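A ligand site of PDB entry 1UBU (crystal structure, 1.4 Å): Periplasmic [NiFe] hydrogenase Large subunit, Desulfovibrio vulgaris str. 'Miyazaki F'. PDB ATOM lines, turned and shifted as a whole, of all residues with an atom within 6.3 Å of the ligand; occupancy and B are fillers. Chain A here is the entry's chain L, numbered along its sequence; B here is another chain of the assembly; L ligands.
N of Pro 460 lies close to O2 of the ligand (3.5 Å).
Thr 69 touches the ligand.
Ala 459 touches the ligand (CB to O2, 3.4 Å).
Leu 464 touches the ligand (CD2 to O3, 3.5 Å).
CG1 of Val 482 touches O3 of the ligand, at 3.5 Å.
CD of Pro 483 touches O3 of the ligand, 3.4 Å away.
13 residues have an atom within 4 Å of the ligand: Cys 63, Cys 66, Thr 69, His 70, Ala 459, Pro 460, Arg 461, Leu 464, Val 482, Pro 483, Ser 484, Cys 528 and Cys 531.
The nearest printed residue that does not touch the ligand is Asp 105 (4.7 Å).
N of Cys 528 lies within hydrogen-bond range of OG of Ser 484 (3.0 Å).
The side-chain carboxylate of Glu 16 sits close to the side-chain sulfur of Cys 528, at 3.3 Å.
O of Cys 66 lies within hydrogen-bond range of OG1 of Thr 69 (2.8 Å).
The side-chain sulfur (SG) of Cys 63 sits close to the backbone NH (N) of Val 65.
A ring nitrogen (NE2) of His 70 lies close to the side-chain sulfur of Cys 531 (3.3 Å).
The guanidinium group of Arg 461 lies within salt-bridge range of the side-chain carboxylate of Asp 105 (2.9 Å).
NH2 of Arg 461 is in salt-bridge range of OD2 of Asp 526 (2.8 Å).
The backbone carbonyl oxygen (O) of Val 482 is in hydrogen-bond range of the side-chain hydroxyl (OG1) of Thr 485, at 3.0 Å.
The side-chain sulfur (SG) of Cys 528 binds a nickel atom (NI1) of the ligand, 2.2 Å away.
SG of Cys 66 is bound to NI1 of the ligand, 2.3 Å away.
The side-chain sulfur (SG) of Cys 63 is bound to a nickel atom (NI1) of the ligand (2.3 Å).
The side-chain sulfur (SG) of Cys 531 binds an iron atom (FE1) of the ligand (2.3 Å).
The backbone NH of Ser 484 lies within hydrogen-bond range of an oxygen (O1) of the ligand (2.9 Å).
An oxygen (O1) of the ligand is in hydrogen-bond range of the side-chain hydroxyl (OG) of Ser 484 (2.6 Å).
An oxygen (O2) of the ligand lies within hydrogen-bond range of the backbone NH (N) of Arg 461.
NH1 of Arg 461 lies within hydrogen-bond range of O2 of the ligand (3.1 Å).
O3 of the ligand lies close to NE2 of His 70, at 3.5 Å.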
ATOM      1  N   GLU A  16      -5.747 -13.377  16.570  1.00  0.00           N
ATOM      2  CA  GLU A  16      -4.991 -14.342  15.815  1.00  0.00           C
ATOM      3  C   GLU A  16      -5.267 -15.704  16.480  1.00  0.00           C
ATOM      4  O   GLU A  16      -5.122 -15.915  17.667  1.00  0.00           O
ATOM      5  CB  GLU A  16      -3.496 -14.043  15.803  1.00  0.00           C
ATOM      6  CG  GLU A  16      -2.577 -14.836  14.897  1.00  0.00           C
ATOM      7  CD  GLU A  16      -2.444 -16.311  15.167  1.00  0.00           C
ATOM      8  OE1 GLU A  16      -2.534 -17.180  14.286  1.00  0.00           O
ATOM      9  OE2 GLU A  16      -2.470 -16.589  16.385  1.00  0.00           O
ATOM     10  N   THR A  62       5.909 -19.018  14.136  1.00  0.00           N
ATOM     11  CA  THR A  62       4.990 -19.082  15.266  1.00  0.00           C
ATOM     12  C   THR A  62       3.784 -18.174  15.004  1.00  0.00           C
ATOM     13  O   THR A  62       2.652 -18.493  15.316  1.00  0.00           O
ATOM     14  CB  THR A  62       5.646 -18.620  16.585  1.00  0.00           C
ATOM     15  OG1 THR A  62       6.690 -19.572  16.943  1.00  0.00           O
ATOM     16  CG2 THR A  62       4.626 -18.575  17.693  1.00  0.00           C
ATOM     17  N   CYS A  63       4.080 -17.007  14.418  1.00  0.00           N
ATOM     18  CA  CYS A  63       3.042 -16.006  14.260  1.00  0.00           C
ATOM     19  C   CYS A  63       3.420 -14.950  13.209  1.00  0.00           C
ATOM     20  O   CYS A  63       4.533 -14.428  13.256  1.00  0.00           O
ATOM     21  CB  CYS A  63       2.798 -15.357  15.594  1.00  0.00           C
ATOM     22  SG  CYS A  63       1.365 -14.183  15.522  1.00  0.00           S
ATOM     23  N   GLY A  64       2.503 -14.680  12.286  1.00  0.00           N
ATOM     24  CA  GLY A  64       2.677 -13.645  11.256  1.00  0.00           C
ATOM     25  C   GLY A  64       1.996 -12.325  11.593  1.00  0.00           C
ATOM     26  O   GLY A  64       2.122 -11.387  10.790  1.00  0.00           O
ATOM     27  N   VAL A  65       1.252 -12.271  12.693  1.00  0.00           N
ATOM     28  CA  VAL A  65       0.710 -11.010  13.219  1.00  0.00           C
ATOM     29  C   VAL A  65       1.853 -10.327  13.965  1.00  0.00           C
ATOM     30  O   VAL A  65       2.292  -9.251  13.529  1.00  0.00           O
ATOM     31  CB  VAL A  65      -0.521 -11.228  14.087  1.00  0.00           C
ATOM     32  CG1 VAL A  65      -0.975  -9.923  14.724  1.00  0.00           C
ATOM     33  CG2 VAL A  65      -1.643 -11.802  13.232  1.00  0.00           C
ATOM     34  N   CYS A  66       2.347 -10.989  15.011  1.00  0.00           N
ATOM     35  CA  CYS A  66       3.571 -10.535  15.615  1.00  0.00           C
ATOM     36  C   CYS A  66       4.764 -11.111  14.866  1.00  0.00           C
ATOM     37  O   CYS A  66       5.714 -11.675  15.382  1.00  0.00           O
ATOM     38  CB  CYS A  66       3.577 -10.838  17.115  1.00  0.00           C
ATOM     39  SG  CYS A  66       3.605 -12.580  17.553  1.00  0.00           S
ATOM     40  N   THR A  67       4.766 -10.930  13.558  1.00  0.00           N
ATOM     41  CA  THR A  67       5.901 -11.284  12.738  1.00  0.00           C
ATOM     42  C   THR A  67       7.142 -10.559  13.252  1.00  0.00           C
ATOM     43  O   THR A  67       7.034  -9.585  14.019  1.00  0.00           O
ATOM     44  CB  THR A  67       5.577 -11.003  11.255  1.00  0.00           C
ATOM     45  OG1 THR A  67       6.636 -11.536  10.444  1.00  0.00           O
ATOM     46  CG2 THR A  67       5.466  -9.507  10.940  1.00  0.00           C
ATOM     47  N   THR A  69       8.950 -10.718  15.652  1.00  0.00           N
ATOM     48  CA  THR A  69       9.296 -10.818  17.067  1.00  0.00           C
ATOM     49  C   THR A  69       9.959 -12.131  17.467  1.00  0.00           C
ATOM     50  O   THR A  69      10.875 -12.184  18.273  1.00  0.00           O
ATOM     51  CB  THR A  69       8.046 -10.604  17.968  1.00  0.00           C
ATOM     52  OG1 THR A  69       7.116 -11.646  17.761  1.00  0.00           O
ATOM     53  CG2 THR A  69       7.390  -9.276  17.674  1.00  0.00           C
ATOM     54  N   HIS A  70       9.514 -13.237  16.907  1.00  0.00           N
ATOM     55  CA  HIS A  70      10.133 -14.517  17.231  1.00  0.00           C
ATOM     56  C   HIS A  70      11.459 -14.716  16.522  1.00  0.00           C
ATOM     57  O   HIS A  70      12.346 -15.354  17.102  1.00  0.00           O
ATOM     58  CB  HIS A  70       9.178 -15.677  16.913  1.00  0.00           C
ATOM     59  CG  HIS A  70       7.974 -15.721  17.766  1.00  0.00           C
ATOM     60  ND1 HIS A  70       7.995 -16.315  19.021  1.00  0.00           N
ATOM     61  CD2 HIS A  70       6.717 -15.247  17.596  1.00  0.00           C
ATOM     62  CE1 HIS A  70       6.792 -16.210  19.571  1.00  0.00           C
ATOM     63  NE2 HIS A  70       6.002 -15.562  18.706  1.00  0.00           N
ATOM     64  N   ASP A 105       1.218  -3.179  14.491  1.00  0.00           N
ATOM     65  CA  ASP A 105       0.447  -4.168  15.222  1.00  0.00           C
ATOM     66  C   ASP A 105      -0.664  -3.510  16.048  1.00  0.00           C
ATOM     67  O   ASP A 105      -1.841  -3.870  15.939  1.00  0.00           O
ATOM     68  CB  ASP A 105       1.406  -5.010  16.088  1.00  0.00           C
ATOM     69  CG  ASP A 105       0.843  -6.319  16.571  1.00  0.00           C
ATOM     70  OD1 ASP A 105      -0.395  -6.497  16.661  1.00  0.00           O
ATOM     71  OD2 ASP A 105       1.746  -7.190  16.812  1.00  0.00           O
ATOM     72  N   ALA A 459       7.316  -8.012  23.253  1.00  0.00           N
ATOM     73  CA  ALA A 459       6.557  -7.960  22.003  1.00  0.00           C
ATOM     74  C   ALA A 459       5.319  -7.118  22.182  1.00  0.00           C
ATOM     75  O   ALA A 459       5.008  -6.735  23.319  1.00  0.00           O
ATOM     76  CB  ALA A 459       6.213  -9.392  21.550  1.00  0.00           C
ATOM     77  N   PRO A 460       4.596  -6.792  21.120  1.00  0.00           N
ATOM     78  CA  PRO A 460       3.347  -6.032  21.296  1.00  0.00           C
ATOM     79  C   PRO A 460       2.366  -6.651  22.295  1.00  0.00           C
ATOM     80  O   PRO A 460       1.524  -5.895  22.826  1.00  0.00           O
ATOM     81  CB  PRO A 460       2.796  -5.975  19.849  1.00  0.00           C
ATOM     82  CG  PRO A 460       4.057  -5.974  19.034  1.00  0.00           C
ATOM     83  CD  PRO A 460       4.926  -7.003  19.716  1.00  0.00           C
ATOM     84  N   ARG A 461       2.404  -7.955  22.566  1.00  0.00           N
ATOM     85  CA  ARG A 461       1.524  -8.604  23.554  1.00  0.00           C
ATOM     86  C   ARG A 461       2.224  -8.921  24.891  1.00  0.00           C
ATOM     87  O   ARG A 461       1.588  -9.457  25.797  1.00  0.00           O
ATOM     88  CB  ARG A 461       0.878  -9.863  22.954  1.00  0.00           C
ATOM     89  CG  ARG A 461      -0.107  -9.507  21.843  1.00  0.00           C
ATOM     90  CD  ARG A 461      -0.430 -10.665  20.871  1.00  0.00           C
ATOM     91  NE  ARG A 461      -1.184 -10.042  19.798  1.00  0.00           N
ATOM     92  CZ  ARG A 461      -0.675  -9.342  18.800  1.00  0.00           C
ATOM     93  NH1 ARG A 461       0.613  -9.153  18.610  1.00  0.00           N
ATOM     94  NH2 ARG A 461      -1.518  -8.802  17.909  1.00  0.00           N
ATOM     95  N   GLY A 462       3.539  -8.607  24.980  1.00  0.00           N
ATOM     96  CA  GLY A 462       4.236  -8.726  26.253  1.00  0.00           C
ATOM     97  C   GLY A 462       5.488  -9.570  26.235  1.00  0.00           C
ATOM     98  O   GLY A 462       6.180  -9.677  25.225  1.00  0.00           O
ATOM     99  N   GLY A 463       5.836 -10.142  27.413  1.00  0.00           N
ATOM    100  CA  GLY A 463       7.154 -10.713  27.519  1.00  0.00           C
ATOM    101  C   GLY A 463       7.312 -12.051  26.833  1.00  0.00           C
ATOM    102  O   GLY A 463       6.711 -13.064  27.260  1.00  0.00           O
ATOM    103  N   LEU A 464       8.169 -12.059  25.831  1.00  0.00           N
ATOM    104  CA  LEU A 464       8.498 -13.203  25.028  1.00  0.00           C
ATOM    105  C   LEU A 464       9.869 -13.759  25.370  1.00  0.00           C
ATOM    106  O   LEU A 464      10.780 -12.935  25.447  1.00  0.00           O
ATOM    107  CB  LEU A 464       8.428 -12.835  23.540  1.00  0.00           C
ATOM    108  CG  LEU A 464       8.979 -13.841  22.543  1.00  0.00           C
ATOM    109  CD1 LEU A 464       8.190 -15.171  22.570  1.00  0.00           C
ATOM    110  CD2 LEU A 464       8.985 -13.241  21.129  1.00  0.00           C
ATOM    111  N   VAL A 482       5.531 -17.634  25.521  1.00  0.00           N
ATOM    112  CA  VAL A 482       5.149 -16.499  24.685  1.00  0.00           C
ATOM    113  C   VAL A 482       4.138 -15.632  25.415  1.00  0.00           C
ATOM    114  O   VAL A 482       3.441 -16.174  26.313  1.00  0.00           O
ATOM    115  CB  VAL A 482       4.591 -17.082  23.366  1.00  0.00           C
ATOM    116  CG1 VAL A 482       4.280 -16.037  22.333  1.00  0.00           C
ATOM    117  CG2 VAL A 482       5.604 -18.006  22.721  1.00  0.00           C
ATOM    118  N   PRO A 483       4.012 -14.347  25.160  1.00  0.00           N
ATOM    119  CA  PRO A 483       3.098 -13.507  25.962  1.00  0.00           C
ATOM    120  C   PRO A 483       1.679 -14.046  26.061  1.00  0.00           C
ATOM    121  O   PRO A 483       1.156 -14.098  27.198  1.00  0.00           O
ATOM    122  CB  PRO A 483       3.113 -12.143  25.288  1.00  0.00           C
ATOM    123  CG  PRO A 483       4.163 -12.212  24.262  1.00  0.00           C
ATOM    124  CD  PRO A 483       4.818 -13.500  24.304  1.00  0.00           C
ATOM    125  N   SER A 484       1.059 -14.476  24.952  1.00  0.00           N
ATOM    126  CA  SER A 484      -0.313 -14.999  25.097  1.00  0.00           C
ATOM    127  C   SER A 484      -0.358 -16.291  25.907  1.00  0.00           C
ATOM    128  O   SER A 484      -1.435 -16.637  26.394  1.00  0.00           O
ATOM    129  CB  SER A 484      -0.983 -15.182  23.751  1.00  0.00           C
ATOM    130  OG  SER A 484      -1.203 -13.953  23.069  1.00  0.00           O
ATOM    131  N   THR A 485       0.772 -17.003  25.998  1.00  0.00           N
ATOM    132  CA  THR A 485       0.782 -18.155  26.887  1.00  0.00           C
ATOM    133  C   THR A 485       0.556 -17.710  28.342  1.00  0.00           C
ATOM    134  O   THR A 485      -0.254 -18.312  29.049  1.00  0.00           O
ATOM    135  CB  THR A 485       2.118 -18.913  26.769  1.00  0.00           C
ATOM    136  OG1 THR A 485       2.631 -18.971  25.431  1.00  0.00           O
ATOM    137  CG2 THR A 485       1.936 -20.363  27.266  1.00  0.00           C
ATOM    138  N   ASP A 526      -5.617  -8.733  23.374  1.00  0.00           N
ATOM    139  CA  ASP A 526      -4.984  -8.928  22.074  1.00  0.00           C
ATOM    140  C   ASP A 526      -4.453 -10.345  21.953  1.00  0.00           C
ATOM    141  O   ASP A 526      -3.276 -10.592  21.710  1.00  0.00           O
ATOM    142  CB  ASP A 526      -3.911  -7.897  21.854  1.00  0.00           C
ATOM    143  CG  ASP A 526      -3.313  -7.776  20.479  1.00  0.00           C
ATOM    144  OD1 ASP A 526      -2.344  -6.961  20.406  1.00  0.00           O
ATOM    145  OD2 ASP A 526      -3.783  -8.466  19.532  1.00  0.00           O
ATOM    146  N   PRO A 527      -5.314 -11.357  22.091  1.00  0.00           N
ATOM    147  CA  PRO A 527      -4.854 -12.749  22.053  1.00  0.00           C
ATOM    148  C   PRO A 527      -4.234 -13.176  20.750  1.00  0.00           C
ATOM    149  O   PRO A 527      -4.664 -12.831  19.652  1.00  0.00           O
ATOM    150  CB  PRO A 527      -6.159 -13.545  22.220  1.00  0.00           C
ATOM    151  CG  PRO A 527      -7.135 -12.607  22.877  1.00  0.00           C
ATOM    152  CD  PRO A 527      -6.776 -11.264  22.257  1.00  0.00           C
ATOM    153  N   CYS A 528      -3.206 -14.028  20.883  1.00  0.00           N
ATOM    154  CA  CYS A 528      -2.544 -14.647  19.720  1.00  0.00           C
ATOM    155  C   CYS A 528      -2.369 -16.126  20.023  1.00  0.00           C
ATOM    156  O   CYS A 528      -1.481 -16.413  20.842  1.00  0.00           O
ATOM    157  CB  CYS A 528      -1.261 -13.866  19.493  1.00  0.00           C
ATOM    158  SG  CYS A 528      -0.499 -14.359  17.921  1.00  0.00           S
ATOM    159  N   ILE A 529      -3.202 -16.961  19.457  1.00  0.00           N
ATOM    160  CA  ILE A 529      -3.163 -18.349  19.896  1.00  0.00           C
ATOM    161  C   ILE A 529      -2.095 -19.178  19.205  1.00  0.00           C
ATOM    162  O   ILE A 529      -1.636 -20.163  19.802  1.00  0.00           O
ATOM    163  CB  ILE A 529      -4.564 -18.977  19.730  1.00  0.00           C
ATOM    164  CG1 ILE A 529      -5.718 -18.085  20.196  1.00  0.00           C
ATOM    165  CG2 ILE A 529      -4.586 -20.331  20.422  1.00  0.00           C
ATOM    166  CD1 ILE A 529      -5.539 -17.598  21.619  1.00  0.00           C
ATOM    167  N   ALA A 530      -1.694 -18.800  17.997  1.00  0.00           N
ATOM    168  CA  ALA A 530      -0.558 -19.449  17.357  1.00  0.00           C
ATOM    169  C   ALA A 530       0.696 -19.164  18.170  1.00  0.00           C
ATOM    170  O   ALA A 530       1.522 -20.031  18.451  1.00  0.00           O
ATOM    171  CB  ALA A 530      -0.448 -18.928  15.944  1.00  0.00           C
ATOM    172  N   CYS A 531       0.798 -17.937  18.634  1.00  0.00           N
ATOM    173  CA  CYS A 531       1.842 -17.559  19.581  1.00  0.00           C
ATOM    174  C   CYS A 531       1.743 -18.375  20.864  1.00  0.00           C
ATOM    175  O   CYS A 531       2.716 -18.948  21.345  1.00  0.00           O
ATOM    176  CB  CYS A 531       1.751 -16.085  19.963  1.00  0.00           C
ATOM    177  SG  CYS A 531       2.781 -15.030  18.914  1.00  0.00           S
ATOM    178  N   GLY A 532       0.541 -18.409  21.467  1.00  0.00           N
ATOM    179  CA  GLY A 532       0.475 -19.009  22.800  1.00  0.00           C
ATOM    180  C   GLY A 532       0.806 -20.482  22.837  1.00  0.00           C
ATOM    181  O   GLY A 532       1.391 -20.966  23.826  1.00  0.00           O
ATOM    182  N   CYS B  17      -0.103 -19.457  10.915  1.00  0.00           N
ATOM    183  CA  CYS B  17       0.432 -18.442  11.765  1.00  0.00           C
ATOM    184  C   CYS B  17      -0.211 -17.082  11.485  1.00  0.00           C
ATOM    185  O   CYS B  17       0.114 -16.125  12.187  1.00  0.00           O
ATOM    186  CB  CYS B  17       1.932 -18.321  11.567  1.00  0.00           C
ATOM    187  SG  CYS B  17       2.439 -17.399  10.075  1.00  0.00           S
HETATM  188 NI1  LIG L   1       1.514 -13.421  17.656  1.00  0.00          NI
HETATM  189 FE1  LIG L   1       2.991 -12.863  19.730  1.00  0.00          FE
HETATM  190  C1  LIG L   1       1.943 -13.284  21.346  1.00  0.00           C
HETATM  191  C2  LIG L   1       3.043 -10.899  20.143  1.00  0.00           C
HETATM  192  C3  LIG L   1       4.565 -12.960  20.467  1.00  0.00           C
HETATM  193  O1  LIG L   1       1.175 -13.483  22.209  1.00  0.00           O
HETATM  194  O2  LIG L   1       3.077  -9.829  20.409  1.00  0.00           O
HETATM  195  O3  LIG L   1       5.539 -13.035  21.060  1.00  0.00           O
